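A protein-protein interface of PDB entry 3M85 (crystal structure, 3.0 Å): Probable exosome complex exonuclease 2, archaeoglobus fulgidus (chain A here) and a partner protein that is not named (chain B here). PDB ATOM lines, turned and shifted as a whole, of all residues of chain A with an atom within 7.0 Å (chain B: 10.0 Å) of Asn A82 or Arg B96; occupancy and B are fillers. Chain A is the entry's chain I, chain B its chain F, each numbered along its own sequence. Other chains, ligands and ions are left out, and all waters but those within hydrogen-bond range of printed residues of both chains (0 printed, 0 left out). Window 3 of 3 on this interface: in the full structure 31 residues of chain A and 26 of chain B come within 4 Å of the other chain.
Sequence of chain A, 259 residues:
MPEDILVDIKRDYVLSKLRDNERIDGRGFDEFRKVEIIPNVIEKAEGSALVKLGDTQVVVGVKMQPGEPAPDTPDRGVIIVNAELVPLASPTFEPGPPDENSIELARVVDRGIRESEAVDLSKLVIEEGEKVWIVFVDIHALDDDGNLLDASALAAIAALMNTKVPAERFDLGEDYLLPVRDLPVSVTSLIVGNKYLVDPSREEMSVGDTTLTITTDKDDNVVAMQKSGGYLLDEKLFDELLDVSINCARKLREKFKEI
The side-chain amino group (NZ) of Lys B103 is in salt-bridge range of the side-chain carboxylate (OE2) of Glu A104, at 3.4 Å. The guanidinium group (NH1) of Arg B96 sits close to the side-chain amide nitrogen (ND2) of Asn A82 (2.9 Å). OE2 of Glu B100 lies within salt-bridge range of NH2 of Arg A107 (3.6 Å).
O of Asn A82 sits at hydrogen-bond distance from N of Ile A139, at 2.7 Å. The backbone carbonyl oxygen (O) of Val A137 is in hydrogen-bond range of the backbone NH (N) of Asn A82, at 3.0 Å. The side-chain hydroxyl (OH) of Tyr B79 lies within hydrogen-bond range of the guanidinium group (NH1) of Arg B97. The side-chain carboxylate of Glu B100 sits close to the side-chain amide oxygen of Gln B205 (3.4 Å).
CD of Arg B96 touches CG2 of Ile A103, 3.5 Å away. OE1 of Glu B100 touches OE2 of Glu A104 (3.5 Å). NE of Arg A107 touches O of Arg B96, at 3.96 Å. Arg B97 touches Arg A107 (CB to NH1, 3.6 Å).
Of chain B, only Arg B96 (2.4 Å) comes within 4 Å of Asn A82. Of the printed residues of chain A, Arg B96 touches Asn A82 (2.4 Å), Ile A103 (3.5 Å) and Arg A107 (3.96 Å). No residue of chain B comes within 4 Å of Ala A83. No residue of chain B comes within 4 Å of Asp A138. No residue of chain B comes within 4 Å of Ile A139. Of the printed residues of chain B, Arg A107 touches Arg B96 (3.96 Å), Arg B97 (3.6 Å) and Glu B100 (3.5 Å). Of the printed residues of chain A, Arg B97 touches Arg A107 (3.6 Å). Printed residues of chain B within 4 Å of Glu A104: Glu B100 (3.5 Å) and Lys B103 (3.4 Å). Printed residues of chain A within 4 Å of Lys B103: Glu A104. Ile B99 touches none of the printed residues of chain A. Val A137 touches none of the printed residues of chain B. The nearest printed residue of chain A that does not touch Arg B96 is Val A81 (4.01 Å). The nearest printed residue of chain B that does not touch Arg A107 is Gln B205 (5.8 Å).
Of the 19 printed residues of chain A, 4 touch a printed residue of chain B. Of the 16 printed residues of chain B, 4 touch a printed residue of chain A. Printed residues of chain B that touch a printed residue of chain A: Arg B96, Arg B97, Glu B100 and Lys B103. Among the printed residues, 7 pairs touch across the chains. Among the printed residues, Asp or Glu carboxylates within 4 Å of a Lys or Arg side-chain nitrogen of the other chain: Glu A104 with Lys B103 and Arg A107 with Glu B100.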
ATOM      1  N   VAL A  60      -1.582  17.262  12.959  1.00  0.00           N
ATOM      2  CA  VAL A  60      -1.873  16.248  13.942  1.00  0.00           C
ATOM      3  C   VAL A  60      -0.563  15.540  14.226  1.00  0.00           C
ATOM      4  O   VAL A  60       0.237  15.314  13.317  1.00  0.00           O
ATOM      5  CB  VAL A  60      -2.898  15.246  13.416  1.00  0.00           C
ATOM      6  CG1 VAL A  60      -2.990  14.022  14.341  1.00  0.00           C
ATOM      7  CG2 VAL A  60      -4.237  15.933  13.256  1.00  0.00           C
ATOM      8  N   ILE A  80      -6.797   7.837  21.842  1.00  0.00           N
ATOM      9  CA  ILE A  80      -7.431   9.003  22.435  1.00  0.00           C
ATOM     10  C   ILE A  80      -7.287  10.258  21.585  1.00  0.00           C
ATOM     11  O   ILE A  80      -6.278  10.959  21.659  1.00  0.00           O
ATOM     12  CB  ILE A  80      -6.836   9.274  23.826  1.00  0.00           C
ATOM     13  CG1 ILE A  80      -7.042   8.052  24.725  1.00  0.00           C
ATOM     14  CG2 ILE A  80      -7.418  10.553  24.435  1.00  0.00           C
ATOM     15  CD1 ILE A  80      -6.301   8.131  26.030  1.00  0.00           C
ATOM     16  N   VAL A  81      -8.312  10.555  20.800  1.00  0.00           N
ATOM     17  CA  VAL A  81      -8.287  11.736  19.950  1.00  0.00           C
ATOM     18  C   VAL A  81      -8.701  13.014  20.691  1.00  0.00           C
ATOM     19  O   VAL A  81      -9.689  13.041  21.411  1.00  0.00           O
ATOM     20  CB  VAL A  81      -9.160  11.539  18.696  1.00  0.00           C
ATOM     21  CG1 VAL A  81      -8.881  12.634  17.701  1.00  0.00           C
ATOM     22  CG2 VAL A  81      -8.888  10.178  18.066  1.00  0.00           C
ATOM     23  N   ASN A  82      -7.934  14.075  20.489  1.00  0.00           N
ATOM     24  CA  ASN A  82      -8.196  15.373  21.099  1.00  0.00           C
ATOM     25  C   ASN A  82      -7.787  16.499  20.153  1.00  0.00           C
ATOM     26  O   ASN A  82      -6.798  16.376  19.438  1.00  0.00           O
ATOM     27  CB  ASN A  82      -7.392  15.517  22.389  1.00  0.00           C
ATOM     28  CG  ASN A  82      -8.219  15.261  23.619  1.00  0.00           C
ATOM     29  OD1 ASN A  82      -8.652  14.133  23.855  1.00  0.00           O
ATOM     30  ND2 ASN A  82      -8.434  16.307  24.427  1.00  0.00           N
ATOM     31  N   ALA A  83      -8.517  17.606  20.157  1.00  0.00           N
ATOM     32  CA  ALA A  83      -8.168  18.707  19.265  1.00  0.00           C
ATOM     33  C   ALA A  83      -8.097  20.037  19.982  1.00  0.00           C
ATOM     34  O   ALA A  83      -8.827  20.285  20.931  1.00  0.00           O
ATOM     35  CB  ALA A  83      -9.156  18.794  18.110  1.00  0.00           C
ATOM     36  N   GLU A  84      -7.215  20.901  19.519  1.00  0.00           N
ATOM     37  CA  GLU A  84      -7.179  22.254  20.034  1.00  0.00           C
ATOM     38  C   GLU A  84      -7.342  23.258  18.874  1.00  0.00           C
ATOM     39  O   GLU A  84      -6.499  23.337  17.979  1.00  0.00           O
ATOM     40  CB  GLU A  84      -5.884  22.485  20.824  1.00  0.00           C
ATOM     41  N   PRO A  98     -11.507  22.851  25.826  1.00  0.00           N
ATOM     42  CA  PRO A  98     -12.189  22.781  24.523  1.00  0.00           C
ATOM     43  C   PRO A  98     -13.628  23.289  24.598  1.00  0.00           C
ATOM     44  O   PRO A  98     -14.397  22.853  25.453  1.00  0.00           O
ATOM     45  CB  PRO A  98     -12.180  21.278  24.188  1.00  0.00           C
ATOM     46  CG  PRO A  98     -11.137  20.669  25.081  1.00  0.00           C
ATOM     47  CD  PRO A  98     -11.101  21.522  26.321  1.00  0.00           C
ATOM     48  N   SER A 102     -14.663  22.354  19.505  1.00  0.00           N
ATOM     49  CA  SER A 102     -13.397  21.662  19.598  1.00  0.00           C
ATOM     50  C   SER A 102     -13.646  20.216  20.013  1.00  0.00           C
ATOM     51  O   SER A 102     -12.854  19.335  19.725  1.00  0.00           O
ATOM     52  CB  SER A 102     -12.506  22.359  20.611  1.00  0.00           C
ATOM     53  OG  SER A 102     -11.186  21.891  20.509  1.00  0.00           O
ATOM     54  N   ILE A 103     -14.758  19.964  20.692  1.00  0.00           N
ATOM     55  CA  ILE A 103     -15.048  18.610  21.148  1.00  0.00           C
ATOM     56  C   ILE A 103     -15.654  17.728  20.063  1.00  0.00           C
ATOM     57  O   ILE A 103     -15.148  16.644  19.787  1.00  0.00           O
ATOM     58  CB  ILE A 103     -15.889  18.591  22.447  1.00  0.00           C
ATOM     59  CG1 ILE A 103     -15.011  19.038  23.628  1.00  0.00           C
ATOM     60  CG2 ILE A 103     -16.475  17.206  22.692  1.00  0.00           C
ATOM     61  CD1 ILE A 103     -15.582  18.759  24.983  1.00  0.00           C
ATOM     62  N   GLU A 104     -16.721  18.186  19.424  1.00  0.00           N
ATOM     63  CA  GLU A 104     -17.318  17.335  18.419  1.00  0.00           C
ATOM     64  C   GLU A 104     -16.343  17.106  17.275  1.00  0.00           C
ATOM     65  O   GLU A 104     -16.379  16.064  16.635  1.00  0.00           O
ATOM     66  CB  GLU A 104     -18.675  17.850  17.937  1.00  0.00           C
ATOM     67  CG  GLU A 104     -18.637  18.727  16.714  1.00  0.00           C
ATOM     68  CD  GLU A 104     -19.992  18.786  15.996  1.00  0.00           C
ATOM     69  OE1 GLU A 104     -20.032  19.331  14.852  1.00  0.00           O
ATOM     70  OE2 GLU A 104     -20.997  18.276  16.574  1.00  0.00           O
ATOM     71  N   LEU A 105     -15.437  18.039  17.034  1.00  0.00           N
ATOM     72  CA  LEU A 105     -14.471  17.800  15.975  1.00  0.00           C
ATOM     73  C   LEU A 105     -13.645  16.577  16.275  1.00  0.00           C
ATOM     74  O   LEU A 105     -13.458  15.736  15.425  1.00  0.00           O
ATOM     75  CB  LEU A 105     -13.552  18.991  15.744  1.00  0.00           C
ATOM     76  CG  LEU A 105     -12.622  18.807  14.537  1.00  0.00           C
ATOM     77  CD1 LEU A 105     -12.774  19.968  13.580  1.00  0.00           C
ATOM     78  CD2 LEU A 105     -11.170  18.660  14.957  1.00  0.00           C
ATOM     79  N   ALA A 106     -13.141  16.465  17.491  1.00  0.00           N
ATOM     80  CA  ALA A 106     -12.333  15.300  17.833  1.00  0.00           C
ATOM     81  C   ALA A 106     -13.155  13.997  17.901  1.00  0.00           C
ATOM     82  O   ALA A 106     -12.695  12.930  17.479  1.00  0.00           O
ATOM     83  CB  ALA A 106     -11.596  15.538  19.131  1.00  0.00           C
ATOM     84  N   ARG A 107     -14.371  14.082  18.431  1.00  0.00           N
ATOM     85  CA  ARG A 107     -15.179  12.891  18.563  1.00  0.00           C
ATOM     86  C   ARG A 107     -15.511  12.327  17.202  1.00  0.00           C
ATOM     87  O   ARG A 107     -15.682  11.120  17.074  1.00  0.00           O
ATOM     88  CB  ARG A 107     -16.461  13.160  19.341  1.00  0.00           C
ATOM     89  CG  ARG A 107     -16.249  13.888  20.632  1.00  0.00           C
ATOM     90  CD  ARG A 107     -17.502  13.851  21.479  1.00  0.00           C
ATOM     91  NE  ARG A 107     -17.584  12.626  22.268  1.00  0.00           N
ATOM     92  CZ  ARG A 107     -18.596  11.763  22.215  1.00  0.00           C
ATOM     93  NH1 ARG A 107     -18.578  10.677  22.979  1.00  0.00           N
ATOM     94  NH2 ARG A 107     -19.627  11.989  21.405  1.00  0.00           N
ATOM     95  N   ASP A 110     -12.262  10.702  15.773  1.00  0.00           N
ATOM     96  CA  ASP A 110     -12.079   9.474  16.527  1.00  0.00           C
ATOM     97  C   ASP A 110     -13.051   8.386  16.068  1.00  0.00           C
ATOM     98  O   ASP A 110     -12.693   7.206  15.979  1.00  0.00           O
ATOM     99  CB  ASP A 110     -12.220   9.733  18.026  1.00  0.00           C
ATOM    100  CG  ASP A 110     -12.177   8.455  18.837  1.00  0.00           C
ATOM    101  OD1 ASP A 110     -11.087   7.873  19.027  1.00  0.00           O
ATOM    102  OD2 ASP A 110     -13.248   8.015  19.272  1.00  0.00           O
ATOM    103  N   PHE A 136      -1.995   8.475  21.453  1.00  0.00           N
ATOM    104  CA  PHE A 136      -2.537   9.824  21.567  1.00  0.00           C
ATOM    105  C   PHE A 136      -2.522  10.524  20.219  1.00  0.00           C
ATOM    106  O   PHE A 136      -1.457  10.917  19.735  1.00  0.00           O
ATOM    107  CB  PHE A 136      -1.724  10.685  22.542  1.00  0.00           C
ATOM    108  CG  PHE A 136      -1.830  10.274  23.990  1.00  0.00           C
ATOM    109  CD1 PHE A 136      -0.833   9.511  24.585  1.00  0.00           C
ATOM    110  CD2 PHE A 136      -2.897  10.696  24.771  1.00  0.00           C
ATOM    111  CE1 PHE A 136      -0.916   9.161  25.921  1.00  0.00           C
ATOM    112  CE2 PHE A 136      -2.986  10.339  26.110  1.00  0.00           C
ATOM    113  CZ  PHE A 136      -1.996   9.573  26.680  1.00  0.00           C
ATOM    114  N   VAL A 137      -3.704  10.691  19.627  1.00  0.00           N
ATOM    115  CA  VAL A 137      -3.875  11.516  18.439  1.00  0.00           C
ATOM    116  C   VAL A 137      -4.272  12.925  18.867  1.00  0.00           C
ATOM    117  O   VAL A 137      -5.304  13.123  19.476  1.00  0.00           O
ATOM    118  CB  VAL A 137      -4.958  10.932  17.529  1.00  0.00           C
ATOM    119  CG1 VAL A 137      -5.250  11.869  16.369  1.00  0.00           C
ATOM    120  CG2 VAL A 137      -4.538   9.572  17.019  1.00  0.00           C
ATOM    121  N   ASP A 138      -3.458  13.913  18.565  1.00  0.00           N
ATOM    122  CA  ASP A 138      -3.803  15.253  18.987  1.00  0.00           C
ATOM    123  C   ASP A 138      -3.830  16.191  17.788  1.00  0.00           C
ATOM    124  O   ASP A 138      -2.810  16.411  17.152  1.00  0.00           O
ATOM    125  CB  ASP A 138      -2.813  15.762  20.030  1.00  0.00           C
ATOM    126  CG  ASP A 138      -3.368  15.710  21.450  1.00  0.00           C
ATOM    127  OD1 ASP A 138      -3.059  14.731  22.174  1.00  0.00           O
ATOM    128  OD2 ASP A 138      -4.094  16.663  21.847  1.00  0.00           O
ATOM    129  N   ILE A 139      -5.014  16.732  17.496  1.00  0.00           N
ATOM    130  CA  ILE A 139      -5.253  17.627  16.369  1.00  0.00           C
ATOM    131  C   ILE A 139      -5.043  19.090  16.776  1.00  0.00           C
ATOM    132  O   ILE A 139      -5.493  19.512  17.838  1.00  0.00           O
ATOM    133  CB  ILE A 139      -6.697  17.453  15.859  1.00  0.00           C
ATOM    134  CG1 ILE A 139      -6.960  15.999  15.488  1.00  0.00           C
ATOM    135  CG2 ILE A 139      -6.964  18.355  14.672  1.00  0.00           C
ATOM    136  CD1 ILE A 139      -8.409  15.704  15.206  1.00  0.00           C
ATOM    137  N   HIS A 140      -4.386  19.868  15.921  1.00  0.00           N
ATOM    138  CA  HIS A 140      -4.033  21.232  16.274  1.00  0.00           C
ATOM    139  C   HIS A 140      -4.197  22.169  15.090  1.00  0.00           C
ATOM    140  O   HIS A 140      -3.333  22.262  14.226  1.00  0.00           O
ATOM    141  CB  HIS A 140      -2.591  21.267  16.743  1.00  0.00           C
ATOM    142  CG  HIS A 140      -2.278  22.406  17.661  1.00  0.00           C
ATOM    143  ND1 HIS A 140      -2.126  23.702  17.212  1.00  0.00           N
ATOM    144  CD2 HIS A 140      -2.060  22.437  18.995  1.00  0.00           C
ATOM    145  CE1 HIS A 140      -1.845  24.486  18.236  1.00  0.00           C
ATOM    146  NE2 HIS A 140      -1.792  23.746  19.329  1.00  0.00           N
ATOM    147  N   TYR B  79     -28.704  17.865  28.749  1.00  0.00           N
ATOM    148  CA  TYR B  79     -28.951  16.432  28.913  1.00  0.00           C
ATOM    149  C   TYR B  79     -27.985  15.877  29.950  1.00  0.00           C
ATOM    150  O   TYR B  79     -26.773  16.019  29.808  1.00  0.00           O
ATOM    151  CB  TYR B  79     -28.703  15.732  27.579  1.00  0.00           C
ATOM    152  CG  TYR B  79     -28.501  14.228  27.651  1.00  0.00           C
ATOM    153  CD1 TYR B  79     -29.499  13.363  27.222  1.00  0.00           C
ATOM    154  CD2 TYR B  79     -27.307  13.677  28.112  1.00  0.00           C
ATOM    155  CE1 TYR B  79     -29.329  11.993  27.259  1.00  0.00           C
ATOM    156  CE2 TYR B  79     -27.128  12.303  28.154  1.00  0.00           C
ATOM    157  CZ  TYR B  79     -28.148  11.465  27.725  1.00  0.00           C
ATOM    158  OH  TYR B  79     -28.003  10.095  27.751  1.00  0.00           O
ATOM    159  N   LYS B  90     -21.789   6.870  38.009  1.00  0.00           N
ATOM    160  CA  LYS B  90     -21.181   7.867  37.132  1.00  0.00           C
ATOM    161  C   LYS B  90     -20.926   9.176  37.873  1.00  0.00           C
ATOM    162  O   LYS B  90     -21.847   9.727  38.467  1.00  0.00           O
ATOM    163  CB  LYS B  90     -22.117   8.147  35.957  1.00  0.00           C
ATOM    164  CG  LYS B  90     -21.465   8.906  34.819  1.00  0.00           C
ATOM    165  CD  LYS B  90     -22.477   9.301  33.764  1.00  0.00           C
ATOM    166  CE  LYS B  90     -23.312  10.453  34.255  1.00  0.00           C
ATOM    167  NZ  LYS B  90     -22.462  11.656  34.488  1.00  0.00           N
ATOM    168  N   ARG B  91     -19.694   9.682  37.829  1.00  0.00           N
ATOM    169  CA  ARG B  91     -19.405  11.001  38.399  1.00  0.00           C
ATOM    170  C   ARG B  91     -20.445  11.982  37.895  1.00  0.00           C
ATOM    171  O   ARG B  91     -20.830  11.935  36.728  1.00  0.00           O
ATOM    172  CB  ARG B  91     -18.031  11.524  37.961  1.00  0.00           C
ATOM    173  CG  ARG B  91     -16.822  10.654  38.296  1.00  0.00           C
ATOM    174  CD  ARG B  91     -15.532  11.305  37.781  1.00  0.00           C
ATOM    175  NE  ARG B  91     -14.372  10.430  37.944  1.00  0.00           N
ATOM    176  CZ  ARG B  91     -13.614   9.982  36.945  1.00  0.00           C
ATOM    177  NH1 ARG B  91     -12.580   9.186  37.206  1.00  0.00           N
ATOM    178  NH2 ARG B  91     -13.880  10.329  35.688  1.00  0.00           N
ATOM    179  N   GLY B  93     -21.553  15.674  36.588  1.00  0.00           N
ATOM    180  CA  GLY B  93     -20.801  16.669  35.856  1.00  0.00           C
ATOM    181  C   GLY B  93     -20.558  16.290  34.418  1.00  0.00           C
ATOM    182  O   GLY B  93     -20.471  15.106  34.078  1.00  0.00           O
ATOM    183  N   PRO B  94     -20.438  17.309  33.562  1.00  0.00           N
ATOM    184  CA  PRO B  94     -20.314  17.149  32.116  1.00  0.00           C
ATOM    185  C   PRO B  94     -19.133  16.274  31.751  1.00  0.00           C
ATOM    186  O   PRO B  94     -18.161  16.169  32.507  1.00  0.00           O
ATOM    187  CB  PRO B  94     -20.050  18.580  31.634  1.00  0.00           C
ATOM    188  CG  PRO B  94     -19.493  19.282  32.837  1.00  0.00           C
ATOM    189  CD  PRO B  94     -20.290  18.717  33.964  1.00  0.00           C
ATOM    190  N   ASP B  95     -19.242  15.642  30.592  1.00  0.00           N
ATOM    191  CA  ASP B  95     -18.125  14.980  29.955  1.00  0.00           C
ATOM    192  C   ASP B  95     -18.290  15.250  28.480  1.00  0.00           C
ATOM    193  O   ASP B  95     -19.285  15.846  28.064  1.00  0.00           O
ATOM    194  CB  ASP B  95     -18.116  13.473  30.228  1.00  0.00           C
ATOM    195  CG  ASP B  95     -19.508  12.870  30.271  1.00  0.00           C
ATOM    196  OD1 ASP B  95     -19.661  11.672  29.942  1.00  0.00           O
ATOM    197  OD2 ASP B  95     -20.453  13.590  30.645  1.00  0.00           O
ATOM    198  N   ARG B  96     -17.309  14.824  27.697  1.00  0.00           N
ATOM    199  CA  ARG B  96     -17.337  15.010  26.262  1.00  0.00           C
ATOM    200  C   ARG B  96     -18.651  14.525  25.662  1.00  0.00           C
ATOM    201  O   ARG B  96     -19.237  15.186  24.791  1.00  0.00           O
ATOM    202  CB  ARG B  96     -16.182  14.240  25.635  1.00  0.00           C
ATOM    203  CG  ARG B  96     -14.828  14.834  25.913  1.00  0.00           C
ATOM    204  CD  ARG B  96     -14.224  15.382  24.642  1.00  0.00           C
ATOM    205  NE  ARG B  96     -12.790  15.486  24.795  1.00  0.00           N
ATOM    206  CZ  ARG B  96     -11.988  14.432  24.810  1.00  0.00           C
ATOM    207  NH1 ARG B  96     -10.684  14.593  24.976  1.00  0.00           N
ATOM    208  NH2 ARG B  96     -12.498  13.212  24.668  1.00  0.00           N
ATOM    209  N   ARG B  97     -19.121  13.367  26.118  1.00  0.00           N
ATOM    210  CA  ARG B  97     -20.320  12.809  25.523  1.00  0.00           C
ATOM    211  C   ARG B  97     -21.542  13.673  25.818  1.00  0.00           C
ATOM    212  O   ARG B  97     -22.469  13.731  25.022  1.00  0.00           O
ATOM    213  CB  ARG B  97     -20.538  11.368  25.960  1.00  0.00           C
ATOM    214  CG  ARG B  97     -21.660  10.659  25.225  1.00  0.00           C
ATOM    215  CD  ARG B  97     -21.803   9.229  25.722  1.00  0.00           C
ATOM    216  NE  ARG B  97     -23.193   8.775  25.706  1.00  0.00           N
ATOM    217  CZ  ARG B  97     -24.077   9.011  26.678  1.00  0.00           C
ATOM    218  NH1 ARG B  97     -25.318   8.554  26.573  1.00  0.00           N
ATOM    219  NH2 ARG B  97     -23.720   9.710  27.755  1.00  0.00           N
ATOM    220  N   SER B  98     -21.539  14.366  26.948  1.00  0.00           N
ATOM    221  CA  SER B  98     -22.695  15.169  27.330  1.00  0.00           C
ATOM    222  C   SER B  98     -22.712  16.513  26.663  1.00  0.00           C
ATOM    223  O   SER B  98     -23.764  16.968  26.223  1.00  0.00           O
ATOM    224  CB  SER B  98     -22.762  15.364  28.835  1.00  0.00           C
ATOM    225  OG  SER B  98     -23.387  14.244  29.427  1.00  0.00           O
ATOM    226  N   ILE B  99     -21.557  17.166  26.614  1.00  0.00           N
ATOM    227  CA  ILE B  99     -21.457  18.439  25.923  1.00  0.00           C
ATOM    228  C   ILE B  99     -22.037  18.229  24.538  1.00  0.00           C
ATOM    229  O   ILE B  99     -22.864  19.000  24.076  1.00  0.00           O
ATOM    230  CB  ILE B  99     -19.993  18.883  25.778  1.00  0.00           C
ATOM    231  CG1 ILE B  99     -19.261  18.779  27.125  1.00  0.00           C
ATOM    232  CG2 ILE B  99     -19.904  20.291  25.173  1.00  0.00           C
ATOM    233  CD1 ILE B  99     -20.037  19.313  28.299  1.00  0.00           C
ATOM    234  N   GLU B 100     -21.621  17.137  23.909  1.00  0.00           N
ATOM    235  CA  GLU B 100     -22.004  16.800  22.539  1.00  0.00           C
ATOM    236  C   GLU B 100     -23.500  16.532  22.336  1.00  0.00           C
ATOM    237  O   GLU B 100     -24.145  17.170  21.494  1.00  0.00           O
ATOM    238  CB  GLU B 100     -21.149  15.614  22.054  1.00  0.00           C
ATOM    239  CG  GLU B 100     -21.852  14.620  21.137  1.00  0.00           C
ATOM    240  CD  GLU B 100     -21.610  14.878  19.656  1.00  0.00           C
ATOM    241  OE1 GLU B 100     -21.582  16.066  19.246  1.00  0.00           O
ATOM    242  OE2 GLU B 100     -21.466  13.878  18.910  1.00  0.00           O
ATOM    243  N   ILE B 101     -24.041  15.581  23.092  1.00  0.00           N
ATOM    244  CA  ILE B 101     -25.464  15.277  23.038  1.00  0.00           C
ATOM    245  C   ILE B 101     -26.294  16.525  23.300  1.00  0.00           C
ATOM    246  O   ILE B 101     -27.264  16.796  22.598  1.00  0.00           O
ATOM    247  CB  ILE B 101     -25.831  14.171  24.040  1.00  0.00           C
ATOM    248  CG1 ILE B 101     -25.182  12.863  23.604  1.00  0.00           C
ATOM    249  CG2 ILE B 101     -27.332  13.999  24.155  1.00  0.00           C
ATOM    250  CD1 ILE B 101     -25.499  11.702  24.503  1.00  0.00           C
ATOM    251  N   SER B 102     -25.903  17.301  24.301  1.00  0.00           N
ATOM    252  CA  SER B 102     -26.610  18.536  24.590  1.00  0.00           C
ATOM    253  C   SER B 102     -26.647  19.405  23.357  1.00  0.00           C
ATOM    254  O   SER B 102     -27.696  19.912  22.985  1.00  0.00           O
ATOM    255  CB  SER B 102     -25.960  19.272  25.750  1.00  0.00           C
ATOM    256  OG  SER B 102     -26.144  18.538  26.946  1.00  0.00           O
ATOM    257  N   LYS B 103     -25.497  19.536  22.709  1.00  0.00           N
ATOM    258  CA  LYS B 103     -25.388  20.324  21.489  1.00  0.00           C
ATOM    259  C   LYS B 103     -26.341  19.849  20.411  1.00  0.00           C
ATOM    260  O   LYS B 103     -27.239  20.589  20.020  1.00  0.00           O
ATOM    261  CB  LYS B 103     -23.956  20.321  20.937  1.00  0.00           C
ATOM    262  CG  LYS B 103     -23.717  21.372  19.847  1.00  0.00           C
ATOM    263  CD  LYS B 103     -22.257  21.449  19.422  1.00  0.00           C
ATOM    264  CE  LYS B 103     -22.110  22.074  18.030  1.00  0.00           C
ATOM    265  NZ  LYS B 103     -22.692  21.206  16.954  1.00  0.00           N
ATOM    266  N   VAL B 104     -26.145  18.625  19.926  1.00  0.00           N
ATOM    267  CA  VAL B 104     -26.924  18.163  18.783  1.00  0.00           C
ATOM    268  C   VAL B 104     -28.405  18.184  19.102  1.00  0.00           C
ATOM    269  O   VAL B 104     -29.213  18.523  18.239  1.00  0.00           O
ATOM    270  CB  VAL B 104     -26.531  16.748  18.305  1.00  0.00           C
ATOM    271  CG1 VAL B 104     -25.030  16.666  18.022  1.00  0.00           C
ATOM    272  CG2 VAL B 104     -26.977  15.682  19.323  1.00  0.00           C
ATOM    273  N   GLN B 205     -27.323  10.848  13.556  1.00  0.00           N
ATOM    274  CA  GLN B 205     -25.958  10.394  13.822  1.00  0.00           C
ATOM    275  C   GLN B 205     -25.814   8.921  13.495  1.00  0.00           C
ATOM    276  O   GLN B 205     -26.766   8.158  13.629  1.00  0.00           O
ATOM    277  CB  GLN B 205     -25.617  10.593  15.281  1.00  0.00           C
ATOM    278  CG  GLN B 205     -25.605  12.040  15.739  1.00  0.00           C
ATOM    279  CD  GLN B 205     -25.118  12.184  17.177  1.00  0.00           C
ATOM    280  OE1 GLN B 205     -23.913  12.080  17.458  1.00  0.00           O
ATOM    281  NE2 GLN B 205     -26.055  12.414  18.097  1.00  0.00           N
